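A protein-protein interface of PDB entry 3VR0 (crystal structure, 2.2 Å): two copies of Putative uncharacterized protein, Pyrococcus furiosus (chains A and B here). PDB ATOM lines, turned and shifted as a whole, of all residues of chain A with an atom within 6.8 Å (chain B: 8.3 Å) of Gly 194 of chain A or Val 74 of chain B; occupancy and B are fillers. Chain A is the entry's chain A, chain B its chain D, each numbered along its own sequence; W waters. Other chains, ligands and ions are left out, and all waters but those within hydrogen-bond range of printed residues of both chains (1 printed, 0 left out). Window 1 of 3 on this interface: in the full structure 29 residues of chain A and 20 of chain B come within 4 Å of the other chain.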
ATOM      1  N   GLU A  37      16.178 -30.481  16.567  1.00  0.00           N
ATOM      2  CA  GLU A  37      16.038 -30.714  17.976  1.00  0.00           C
ATOM      3  C   GLU A  37      14.608 -31.115  18.330  1.00  0.00           C
ATOM      4  O   GLU A  37      13.673 -30.398  17.988  1.00  0.00           O
ATOM      5  CB  GLU A  37      16.435 -29.452  18.747  1.00  0.00           C
ATOM      6  CG  GLU A  37      16.273 -29.551  20.263  1.00  0.00           C
ATOM      7  CD  GLU A  37      14.900 -29.077  20.752  1.00  0.00           C
ATOM      8  OE1 GLU A  37      14.341 -28.139  20.164  1.00  0.00           O
ATOM      9  OE2 GLU A  37      14.372 -29.641  21.726  1.00  0.00           O
ATOM     10  N   THR A 140      14.149 -26.341  15.282  1.00  0.00           N
ATOM     11  CA  THR A 140      13.686 -26.837  16.581  1.00  0.00           C
ATOM     12  C   THR A 140      12.192 -27.189  16.491  1.00  0.00           C
ATOM     13  O   THR A 140      11.416 -26.466  15.863  1.00  0.00           O
ATOM     14  CB  THR A 140      13.958 -25.840  17.750  1.00  0.00           C
ATOM     15  OG1 THR A 140      13.168 -24.666  17.562  1.00  0.00           O
ATOM     16  CG2 THR A 140      15.453 -25.399  17.807  1.00  0.00           C
ATOM     17  N   GLY A 186       6.599 -10.316  21.861  1.00  0.00           N
ATOM     18  CA  GLY A 186       6.754 -10.427  23.298  1.00  0.00           C
ATOM     19  C   GLY A 186       6.358 -11.773  23.865  1.00  0.00           C
ATOM     20  O   GLY A 186       6.516 -11.989  25.044  1.00  0.00           O
ATOM     21  N   GLY A 187       5.840 -12.679  23.041  1.00  0.00           N
ATOM     22  CA  GLY A 187       5.726 -14.112  23.413  1.00  0.00           C
ATOM     23  C   GLY A 187       7.108 -14.766  23.612  1.00  0.00           C
ATOM     24  O   GLY A 187       8.130 -14.192  23.255  1.00  0.00           O
ATOM     25  N   ALA A 188       7.132 -15.970  24.171  1.00  0.00           N
ATOM     26  CA  ALA A 188       8.400 -16.586  24.627  1.00  0.00           C
ATOM     27  C   ALA A 188       8.442 -17.993  24.134  1.00  0.00           C
ATOM     28  O   ALA A 188       7.401 -18.631  24.134  1.00  0.00           O
ATOM     29  CB  ALA A 188       8.466 -16.609  26.160  1.00  0.00           C
ATOM     30  N   ILE A 189       9.628 -18.461  23.742  1.00  0.00           N
ATOM     31  CA  ILE A 189       9.890 -19.898  23.549  1.00  0.00           C
ATOM     32  C   ILE A 189      10.926 -20.350  24.584  1.00  0.00           C
ATOM     33  O   ILE A 189      12.075 -19.905  24.569  1.00  0.00           O
ATOM     34  CB  ILE A 189      10.441 -20.218  22.152  1.00  0.00           C
ATOM     35  CG1 ILE A 189       9.558 -19.522  21.099  1.00  0.00           C
ATOM     36  CG2 ILE A 189      10.551 -21.735  21.965  1.00  0.00           C
ATOM     37  CD1 ILE A 189       9.981 -19.725  19.615  1.00  0.00           C
ATOM     38  N   VAL A 190      10.508 -21.240  25.471  1.00  0.00           N
ATOM     39  CA  VAL A 190      11.281 -21.572  26.666  1.00  0.00           C
ATOM     40  C   VAL A 190      12.102 -22.859  26.440  1.00  0.00           C
ATOM     41  O   VAL A 190      11.595 -23.826  25.859  1.00  0.00           O
ATOM     42  CB  VAL A 190      10.342 -21.765  27.918  1.00  0.00           C
ATOM     43  CG1 VAL A 190      11.158 -22.097  29.176  1.00  0.00           C
ATOM     44  CG2 VAL A 190       9.466 -20.518  28.193  1.00  0.00           C
ATOM     45  N   GLY A 191      13.358 -22.870  26.891  1.00  0.00           N
ATOM     46  CA  GLY A 191      14.205 -24.070  26.828  1.00  0.00           C
ATOM     47  C   GLY A 191      14.923 -24.191  25.476  1.00  0.00           C
ATOM     48  O   GLY A 191      14.932 -23.229  24.702  1.00  0.00           O
ATOM     49  N   ALA A 192      15.475 -25.374  25.196  1.00  0.00           N
ATOM     50  CA  ALA A 192      16.320 -25.615  24.020  1.00  0.00           C
ATOM     51  C   ALA A 192      15.654 -25.171  22.681  1.00  0.00           C
ATOM     52  O   ALA A 192      16.295 -24.652  21.797  1.00  0.00           O
ATOM     53  CB  ALA A 192      16.648 -27.090  23.945  1.00  0.00           C
ATOM     54  N   ALA A 193      14.354 -25.359  22.584  1.00  0.00           N
ATOM     55  CA  ALA A 193      13.623 -25.066  21.345  1.00  0.00           C
ATOM     56  C   ALA A 193      13.737 -23.599  20.982  1.00  0.00           C
ATOM     57  O   ALA A 193      13.596 -23.233  19.802  1.00  0.00           O
ATOM     58  CB  ALA A 193      12.141 -25.506  21.447  1.00  0.00           C
ATOM     59  N   GLY A 194      13.985 -22.767  21.996  1.00  0.00           N
ATOM     60  CA  GLY A 194      14.249 -21.352  21.790  1.00  0.00           C
ATOM     61  C   GLY A 194      15.737 -20.992  21.883  1.00  0.00           C
ATOM     62  O   GLY A 194      16.289 -20.311  20.976  1.00  0.00           O
ATOM     63  N   LEU A 195      16.408 -21.470  22.933  1.00  0.00           N
ATOM     64  CA  LEU A 195      17.840 -21.150  23.151  1.00  0.00           C
ATOM     65  C   LEU A 195      18.764 -21.597  22.050  1.00  0.00           C
ATOM     66  O   LEU A 195      19.715 -20.897  21.733  1.00  0.00           O
ATOM     67  CB  LEU A 195      18.383 -21.721  24.469  1.00  0.00           C
ATOM     68  CG  LEU A 195      17.882 -21.086  25.780  1.00  0.00           C
ATOM     69  CD1 LEU A 195      18.740 -21.539  26.988  1.00  0.00           C
ATOM     70  CD2 LEU A 195      17.895 -19.560  25.686  1.00  0.00           C
ATOM     71  N   LEU A 196      18.529 -22.761  21.455  1.00  0.00           N
ATOM     72  CA  LEU A 196      19.460 -23.163  20.403  1.00  0.00           C
ATOM     73  C   LEU A 196      19.451 -22.139  19.232  1.00  0.00           C
ATOM     74  O   LEU A 196      20.493 -21.851  18.626  1.00  0.00           O
ATOM     75  CB  LEU A 196      19.124 -24.564  19.900  1.00  0.00           C
ATOM     76  CG  LEU A 196      19.411 -25.699  20.912  1.00  0.00           C
ATOM     77  CD1 LEU A 196      18.763 -26.964  20.347  1.00  0.00           C
ATOM     78  CD2 LEU A 196      20.930 -25.923  21.143  1.00  0.00           C
ATOM     79  N   LEU A 197      18.266 -21.616  18.906  1.00  0.00           N
ATOM     80  CA  LEU A 197      18.175 -20.570  17.859  1.00  0.00           C
ATOM     81  C   LEU A 197      18.723 -19.258  18.368  1.00  0.00           C
ATOM     82  O   LEU A 197      19.395 -18.553  17.625  1.00  0.00           O
ATOM     83  CB  LEU A 197      16.715 -20.345  17.404  1.00  0.00           C
ATOM     84  CG  LEU A 197      16.051 -21.568  16.854  1.00  0.00           C
ATOM     85  CD1 LEU A 197      14.555 -21.334  16.649  1.00  0.00           C
ATOM     86  CD2 LEU A 197      16.784 -22.038  15.527  1.00  0.00           C
ATOM     87  N   GLY A 198      18.407 -18.889  19.605  1.00  0.00           N
ATOM     88  CA  GLY A 198      18.785 -17.554  20.099  1.00  0.00           C
ATOM     89  C   GLY A 198      20.303 -17.485  20.283  1.00  0.00           C
ATOM     90  O   GLY A 198      20.969 -16.458  19.969  1.00  0.00           O
ATOM     91  N   ILE A 199      20.865 -18.564  20.821  1.00  0.00           N
ATOM     92  CA  ILE A 199      22.313 -18.604  20.987  1.00  0.00           C
ATOM     93  C   ILE A 199      22.961 -18.829  19.635  1.00  0.00           C
ATOM     94  O   ILE A 199      23.979 -18.177  19.309  1.00  0.00           O
ATOM     95  CB  ILE A 199      22.795 -19.704  21.970  1.00  0.00           C
ATOM     96  CG1 ILE A 199      22.122 -19.503  23.332  1.00  0.00           C
ATOM     97  CG2 ILE A 199      24.341 -19.655  22.042  1.00  0.00           C
ATOM     98  CD1 ILE A 199      22.318 -20.626  24.319  1.00  0.00           C
ATOM     99  N   GLY A 200      22.374 -19.732  18.843  1.00  0.00           N
ATOM    100  CA  GLY A 200      22.876 -19.946  17.473  1.00  0.00           C
ATOM    101  C   GLY A 200      23.043 -18.650  16.686  1.00  0.00           C
ATOM    102  O   GLY A 200      24.114 -18.367  16.085  1.00  0.00           O
ATOM    103  N   SER A 209      11.938 -22.073  14.304  1.00  0.00           N
ATOM    104  CA  SER A 209      11.195 -22.809  15.348  1.00  0.00           C
ATOM    105  C   SER A 209       9.815 -23.272  14.875  1.00  0.00           C
ATOM    106  O   SER A 209       9.021 -22.450  14.405  1.00  0.00           O
ATOM    107  CB  SER A 209      10.989 -21.883  16.544  1.00  0.00           C
ATOM    108  OG  SER A 209       9.957 -22.454  17.315  1.00  0.00           O
ATOM    109  N   MET B  71      16.378 -15.218  32.003  1.00  0.00           N
ATOM    110  CA  MET B  71      15.459 -16.328  31.828  1.00  0.00           C
ATOM    111  C   MET B  71      15.834 -17.080  30.559  1.00  0.00           C
ATOM    112  O   MET B  71      16.218 -16.444  29.529  1.00  0.00           O
ATOM    113  CB  MET B  71      14.012 -15.800  31.781  1.00  0.00           C
ATOM    114  CG  MET B  71      12.977 -16.867  31.467  1.00  0.00           C
ATOM    115  SD  MET B  71      12.988 -18.256  32.713  1.00  0.00           S
ATOM    116  CE  MET B  71      11.821 -19.267  31.822  1.00  0.00           C
ATOM    117  N   HIS B  72      15.688 -18.419  30.628  1.00  0.00           N
ATOM    118  CA  HIS B  72      16.157 -19.306  29.575  1.00  0.00           C
ATOM    119  C   HIS B  72      15.164 -19.428  28.421  1.00  0.00           C
ATOM    120  O   HIS B  72      14.646 -20.512  28.099  1.00  0.00           O
ATOM    121  CB  HIS B  72      16.568 -20.690  30.115  1.00  0.00           C
ATOM    122  CG  HIS B  72      15.516 -21.329  30.971  1.00  0.00           C
ATOM    123  ND1 HIS B  72      15.374 -21.031  32.315  1.00  0.00           N
ATOM    124  CD2 HIS B  72      14.570 -22.259  30.682  1.00  0.00           C
ATOM    125  CE1 HIS B  72      14.364 -21.729  32.803  1.00  0.00           C
ATOM    126  NE2 HIS B  72      13.855 -22.471  31.828  1.00  0.00           N
ATOM    127  N   GLN B  73      14.971 -18.307  27.735  1.00  0.00           N
ATOM    128  CA  GLN B  73      14.010 -18.266  26.635  1.00  0.00           C
ATOM    129  C   GLN B  73      14.429 -17.284  25.570  1.00  0.00           C
ATOM    130  O   GLN B  73      15.269 -16.417  25.815  1.00  0.00           O
ATOM    131  CB  GLN B  73      12.634 -17.871  27.174  1.00  0.00           C
ATOM    132  CG  GLN B  73      12.628 -16.457  27.790  1.00  0.00           C
ATOM    133  CD  GLN B  73      11.328 -16.126  28.492  1.00  0.00           C
ATOM    134  OE1 GLN B  73      10.539 -17.017  28.847  1.00  0.00           O
ATOM    135  NE2 GLN B  73      11.092 -14.865  28.669  1.00  0.00           N
ATOM    136  N   VAL B  74      13.859 -17.436  24.387  1.00  0.00           N
ATOM    137  CA  VAL B  74      13.881 -16.327  23.444  1.00  0.00           C
ATOM    138  C   VAL B  74      12.511 -15.640  23.390  1.00  0.00           C
ATOM    139  O   VAL B  74      11.475 -16.248  23.709  1.00  0.00           O
ATOM    140  CB  VAL B  74      14.241 -16.774  22.007  1.00  0.00           C
ATOM    141  CG1 VAL B  74      15.678 -17.377  21.965  1.00  0.00           C
ATOM    142  CG2 VAL B  74      13.172 -17.731  21.466  1.00  0.00           C
ATOM    143  N   LEU B  75      12.532 -14.403  22.913  1.00  0.00           N
ATOM    144  CA  LEU B  75      11.309 -13.621  22.734  1.00  0.00           C
ATOM    145  C   LEU B  75      10.975 -13.512  21.246  1.00  0.00           C
ATOM    146  O   LEU B  75      11.864 -13.459  20.389  1.00  0.00           O
ATOM    147  CB  LEU B  75      11.508 -12.206  23.285  1.00  0.00           C
ATOM    148  CG  LEU B  75      11.689 -12.048  24.805  1.00  0.00           C
ATOM    149  CD1 LEU B  75      11.880 -10.597  25.148  1.00  0.00           C
ATOM    150  CD2 LEU B  75      10.543 -12.651  25.632  1.00  0.00           C
ATOM    151  N   ILE B  76       9.682 -13.457  20.953  1.00  0.00           N
ATOM    152  CA  ILE B  76       9.209 -13.185  19.616  1.00  0.00           C
ATOM    153  C   ILE B  76       9.343 -11.694  19.343  1.00  0.00           C
ATOM    154  O   ILE B  76       8.764 -10.919  20.058  1.00  0.00           O
ATOM    155  CB  ILE B  76       7.766 -13.610  19.501  1.00  0.00           C
ATOM    156  CG1 ILE B  76       7.643 -15.125  19.767  1.00  0.00           C
ATOM    157  CG2 ILE B  76       7.217 -13.299  18.079  1.00  0.00           C
ATOM    158  CD1 ILE B  76       8.514 -16.052  18.798  1.00  0.00           C
ATOM    159  N   ARG B  77      10.138 -11.284  18.349  1.00  0.00           N
ATOM    160  CA  ARG B  77      10.210  -9.853  17.979  1.00  0.00           C
ATOM    161  C   ARG B  77       9.232  -9.560  16.803  1.00  0.00           C
ATOM    162  O   ARG B  77       8.338 -10.359  16.525  1.00  0.00           O
ATOM    163  CB  ARG B  77      11.646  -9.403  17.610  1.00  0.00           C
ATOM    164  CG  ARG B  77      12.759  -9.875  18.543  1.00  0.00           C
ATOM    165  CD  ARG B  77      12.570  -9.294  19.918  1.00  0.00           C
ATOM    166  NE  ARG B  77      13.815  -9.294  20.659  1.00  0.00           N
ATOM    167  CZ  ARG B  77      13.941  -8.937  21.936  1.00  0.00           C
ATOM    168  NH1 ARG B  77      12.883  -8.518  22.617  1.00  0.00           N
ATOM    169  NH2 ARG B  77      15.146  -8.985  22.522  1.00  0.00           N
ATOM    170  N   VAL B  81      10.476 -13.017  14.175  1.00  0.00           N
ATOM    171  CA  VAL B  81      11.880 -13.204  14.459  1.00  0.00           C
ATOM    172  C   VAL B  81      12.100 -13.578  15.963  1.00  0.00           C
ATOM    173  O   VAL B  81      11.528 -12.961  16.821  1.00  0.00           O
ATOM    174  CB  VAL B  81      12.676 -11.908  14.044  1.00  0.00           C
ATOM    175  CG1 VAL B  81      14.182 -11.931  14.533  1.00  0.00           C
ATOM    176  CG2 VAL B  81      12.638 -11.772  12.496  1.00  0.00           C
ATOM    177  N   VAL B  82      12.867 -14.626  16.266  1.00  0.00           N
ATOM    178  CA  VAL B  82      13.250 -14.906  17.673  1.00  0.00           C
ATOM    179  C   VAL B  82      14.576 -14.266  18.022  1.00  0.00           C
ATOM    180  O   VAL B  82      15.427 -14.101  17.165  1.00  0.00           O
ATOM    181  CB  VAL B  82      13.336 -16.424  18.002  1.00  0.00           C
ATOM    182  CG1 VAL B  82      12.031 -17.112  17.686  1.00  0.00           C
ATOM    183  CG2 VAL B  82      14.465 -17.105  17.251  1.00  0.00           C
ATOM    184  N   GLU B  83      14.743 -13.889  19.288  1.00  0.00           N
ATOM    185  CA  GLU B  83      15.974 -13.338  19.769  1.00  0.00           C
ATOM    186  C   GLU B  83      16.135 -13.559  21.276  1.00  0.00           C
ATOM    187  O   GLU B  83      15.164 -13.439  22.005  1.00  0.00           O
ATOM    188  CB  GLU B  83      15.996 -11.837  19.497  1.00  0.00           C
ATOM    189  CG  GLU B  83      17.355 -11.252  19.822  1.00  0.00           C
ATOM    190  CD  GLU B  83      17.529  -9.842  19.298  1.00  0.00           C
ATOM    191  OE1 GLU B  83      16.559  -9.052  19.377  1.00  0.00           O
ATOM    192  OE2 GLU B  83      18.657  -9.528  18.824  1.00  0.00           O
ATOM    193  N   LEU B  84      17.351 -13.857  21.751  1.00  0.00           N
ATOM    194  CA  LEU B  84      17.556 -13.932  23.202  1.00  0.00           C
ATOM    195  C   LEU B  84      17.075 -12.645  23.884  1.00  0.00           C
ATOM    196  O   LEU B  84      16.953 -11.578  23.244  1.00  0.00           O
ATOM    197  CB  LEU B  84      19.026 -14.142  23.575  1.00  0.00           C
ATOM    198  CG  LEU B  84      19.617 -15.512  23.210  1.00  0.00           C
ATOM    199  CD1 LEU B  84      21.117 -15.429  23.365  1.00  0.00           C
ATOM    200  CD2 LEU B  84      18.984 -16.609  24.094  1.00  0.00           C
ATOM    201  N   MET B  85      16.811 -12.739  25.182  1.00  0.00           N
ATOM    202  CA  MET B  85      16.565 -11.552  25.975  1.00  0.00           C
ATOM    203  C   MET B  85      17.889 -10.793  26.137  1.00  0.00           C
ATOM    204  O   MET B  85      18.984 -11.397  26.262  1.00  0.00           O
ATOM    205  CB  MET B  85      15.965 -11.933  27.310  1.00  0.00           C
ATOM    206  CG  MET B  85      14.627 -12.708  27.144  1.00  0.00           C
ATOM    207  SD  MET B  85      13.741 -12.841  28.698  1.00  0.00           S
ATOM    208  CE  MET B  85      12.936 -11.282  28.654  1.00  0.00           C
ATOM    209  N   ASP B 108      15.125  -5.935  27.662  1.00  0.00           N
ATOM    210  CA  ASP B 108      13.901  -6.760  27.872  1.00  0.00           C
ATOM    211  C   ASP B 108      13.668  -7.122  29.312  1.00  0.00           C
ATOM    212  O   ASP B 108      12.545  -7.451  29.664  1.00  0.00           O
ATOM    213  CB  ASP B 108      13.943  -8.069  27.076  1.00  0.00           C
ATOM    214  CG  ASP B 108      14.318  -7.869  25.639  1.00  0.00           C
ATOM    215  OD1 ASP B 108      13.503  -7.254  24.930  1.00  0.00           O
ATOM    216  OD2 ASP B 108      15.402  -8.338  25.213  1.00  0.00           O
HETATM  217  O   HOH W   1      19.589 -14.026  19.891  1.00  0.00           O
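N of Gly 186 of chain A sits at hydrogen-bond distance from O of Ile 76 of chain B (2.9 Å).
The backbone carbonyl oxygen of Gly 187 of chain A is in hydrogen-bond range of the backbone NH of Ile 76 of chain B.
The backbone NH (N) of Ile 189 of chain A is in hydrogen-bond range of the backbone carbonyl oxygen (O) of Val 74 of chain B, 2.9 Å away.
The backbone NH of Gly 191 of chain A sits at hydrogen-bond distance from the backbone carbonyl oxygen of His 72 of chain B (2.9 Å).
SD of Met 71 of chain B sits at hydrogen-bond distance from ND1 of His 72 of chain B, at 3.7 Å.
SD of Met 85 of chain B is in hydrogen-bond range of NE2 of Gln 73 of chain B, at 3.3 Å.
The backbone NH (N) of Leu 75 of chain B is in hydrogen-bond range of the backbone carbonyl oxygen (O) of Glu 83 of chain B.
The guanidinium group (NH2) of Arg 77 of chain B is in hydrogen-bond range of the backbone carbonyl oxygen (O) of Leu 84 of chain B (3.2 Å).
O of Gly 187 of chain A touches O of Val 74 of chain B, at 3.95 Å.
CB of Ala 188 of chain A touches OE1 of Gln 73 of chain B, 3.4 Å away.
Met 71 of chain B touches Val 190 of chain A.
His 72 of chain B touches Val 190 of chain A.
Gln 73 of chain B touches Val 190 of chain A.
Leu 195 of chain A touches His 72 of chain B (CD2 to C, 3.9 Å).
CD2 of Leu 195 of chain A touches N of Gln 73 of chain B (3.8 Å).
CD2 of Leu 84 of chain B touches CD2 of Leu 195 of chain A, 3.5 Å away.
Gly 198 of chain A touches Val 74 of chain B.
CD1 of Leu 84 of chain B touches O of Gly 198 of chain A (3.6 Å).
Of the printed residues of chain B, Gly 194 of chain A touches Val 74 (3.2 Å).
Printed residues of chain A within 4 Å of His 72 of chain B: Val 190 (3.7 Å), Gly 191 (2.9 Å) and Leu 195 (3.9 Å).
Of the printed residues of chain A, Met 71 of chain B touches Val 190 (3.9 Å).
Printed residues of chain B within 4 Å of Leu 195 of chain A: His 72, Gln 73 and Leu 84.
Printed residues of chain B within 4 Å of Gly 187 of chain A: Val 74 (3.95 Å), Leu 75 (3.3 Å) and Ile 76 (2.9 Å).
Of the printed residues of chain A, Val 82 of chain B touches Ile 189 and Leu 197.
The nearest residue of chain A that does not touch Val 74 of chain B is Leu 195 of chain A (4.3 Å).
Printed residues of chain B that touch a printed residue of chain A: Met 71, His 72, Gln 73, Val 74, Leu 75, Ile 76, Val 82 and Leu 84.
Hydrophobic or aromatic side chains of chain B within 4 Å of the printed part of chain A: Met 71, His 72, Val 74, Leu 75, Ile 76, Val 82 and Leu 84.
Hydrophobic or aromatic side chains of chain A within 4 Å of the printed part of chain B: Ala 188, Ile 189, Val 190, Leu 195 and Leu 197.
Among the printed residues, 20 pairs touch across the chains.
No position is printed for both chains.
Of the 20 pairs that touch across the chains among the printed residues, none has its exchanged pair printed and touching as well.
Water W1 bridges the backbone carbonyl oxygen of Gly 198 of chain A (2.8 Å) and the backbone NH of Leu 84 of chain B (2.9 Å).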
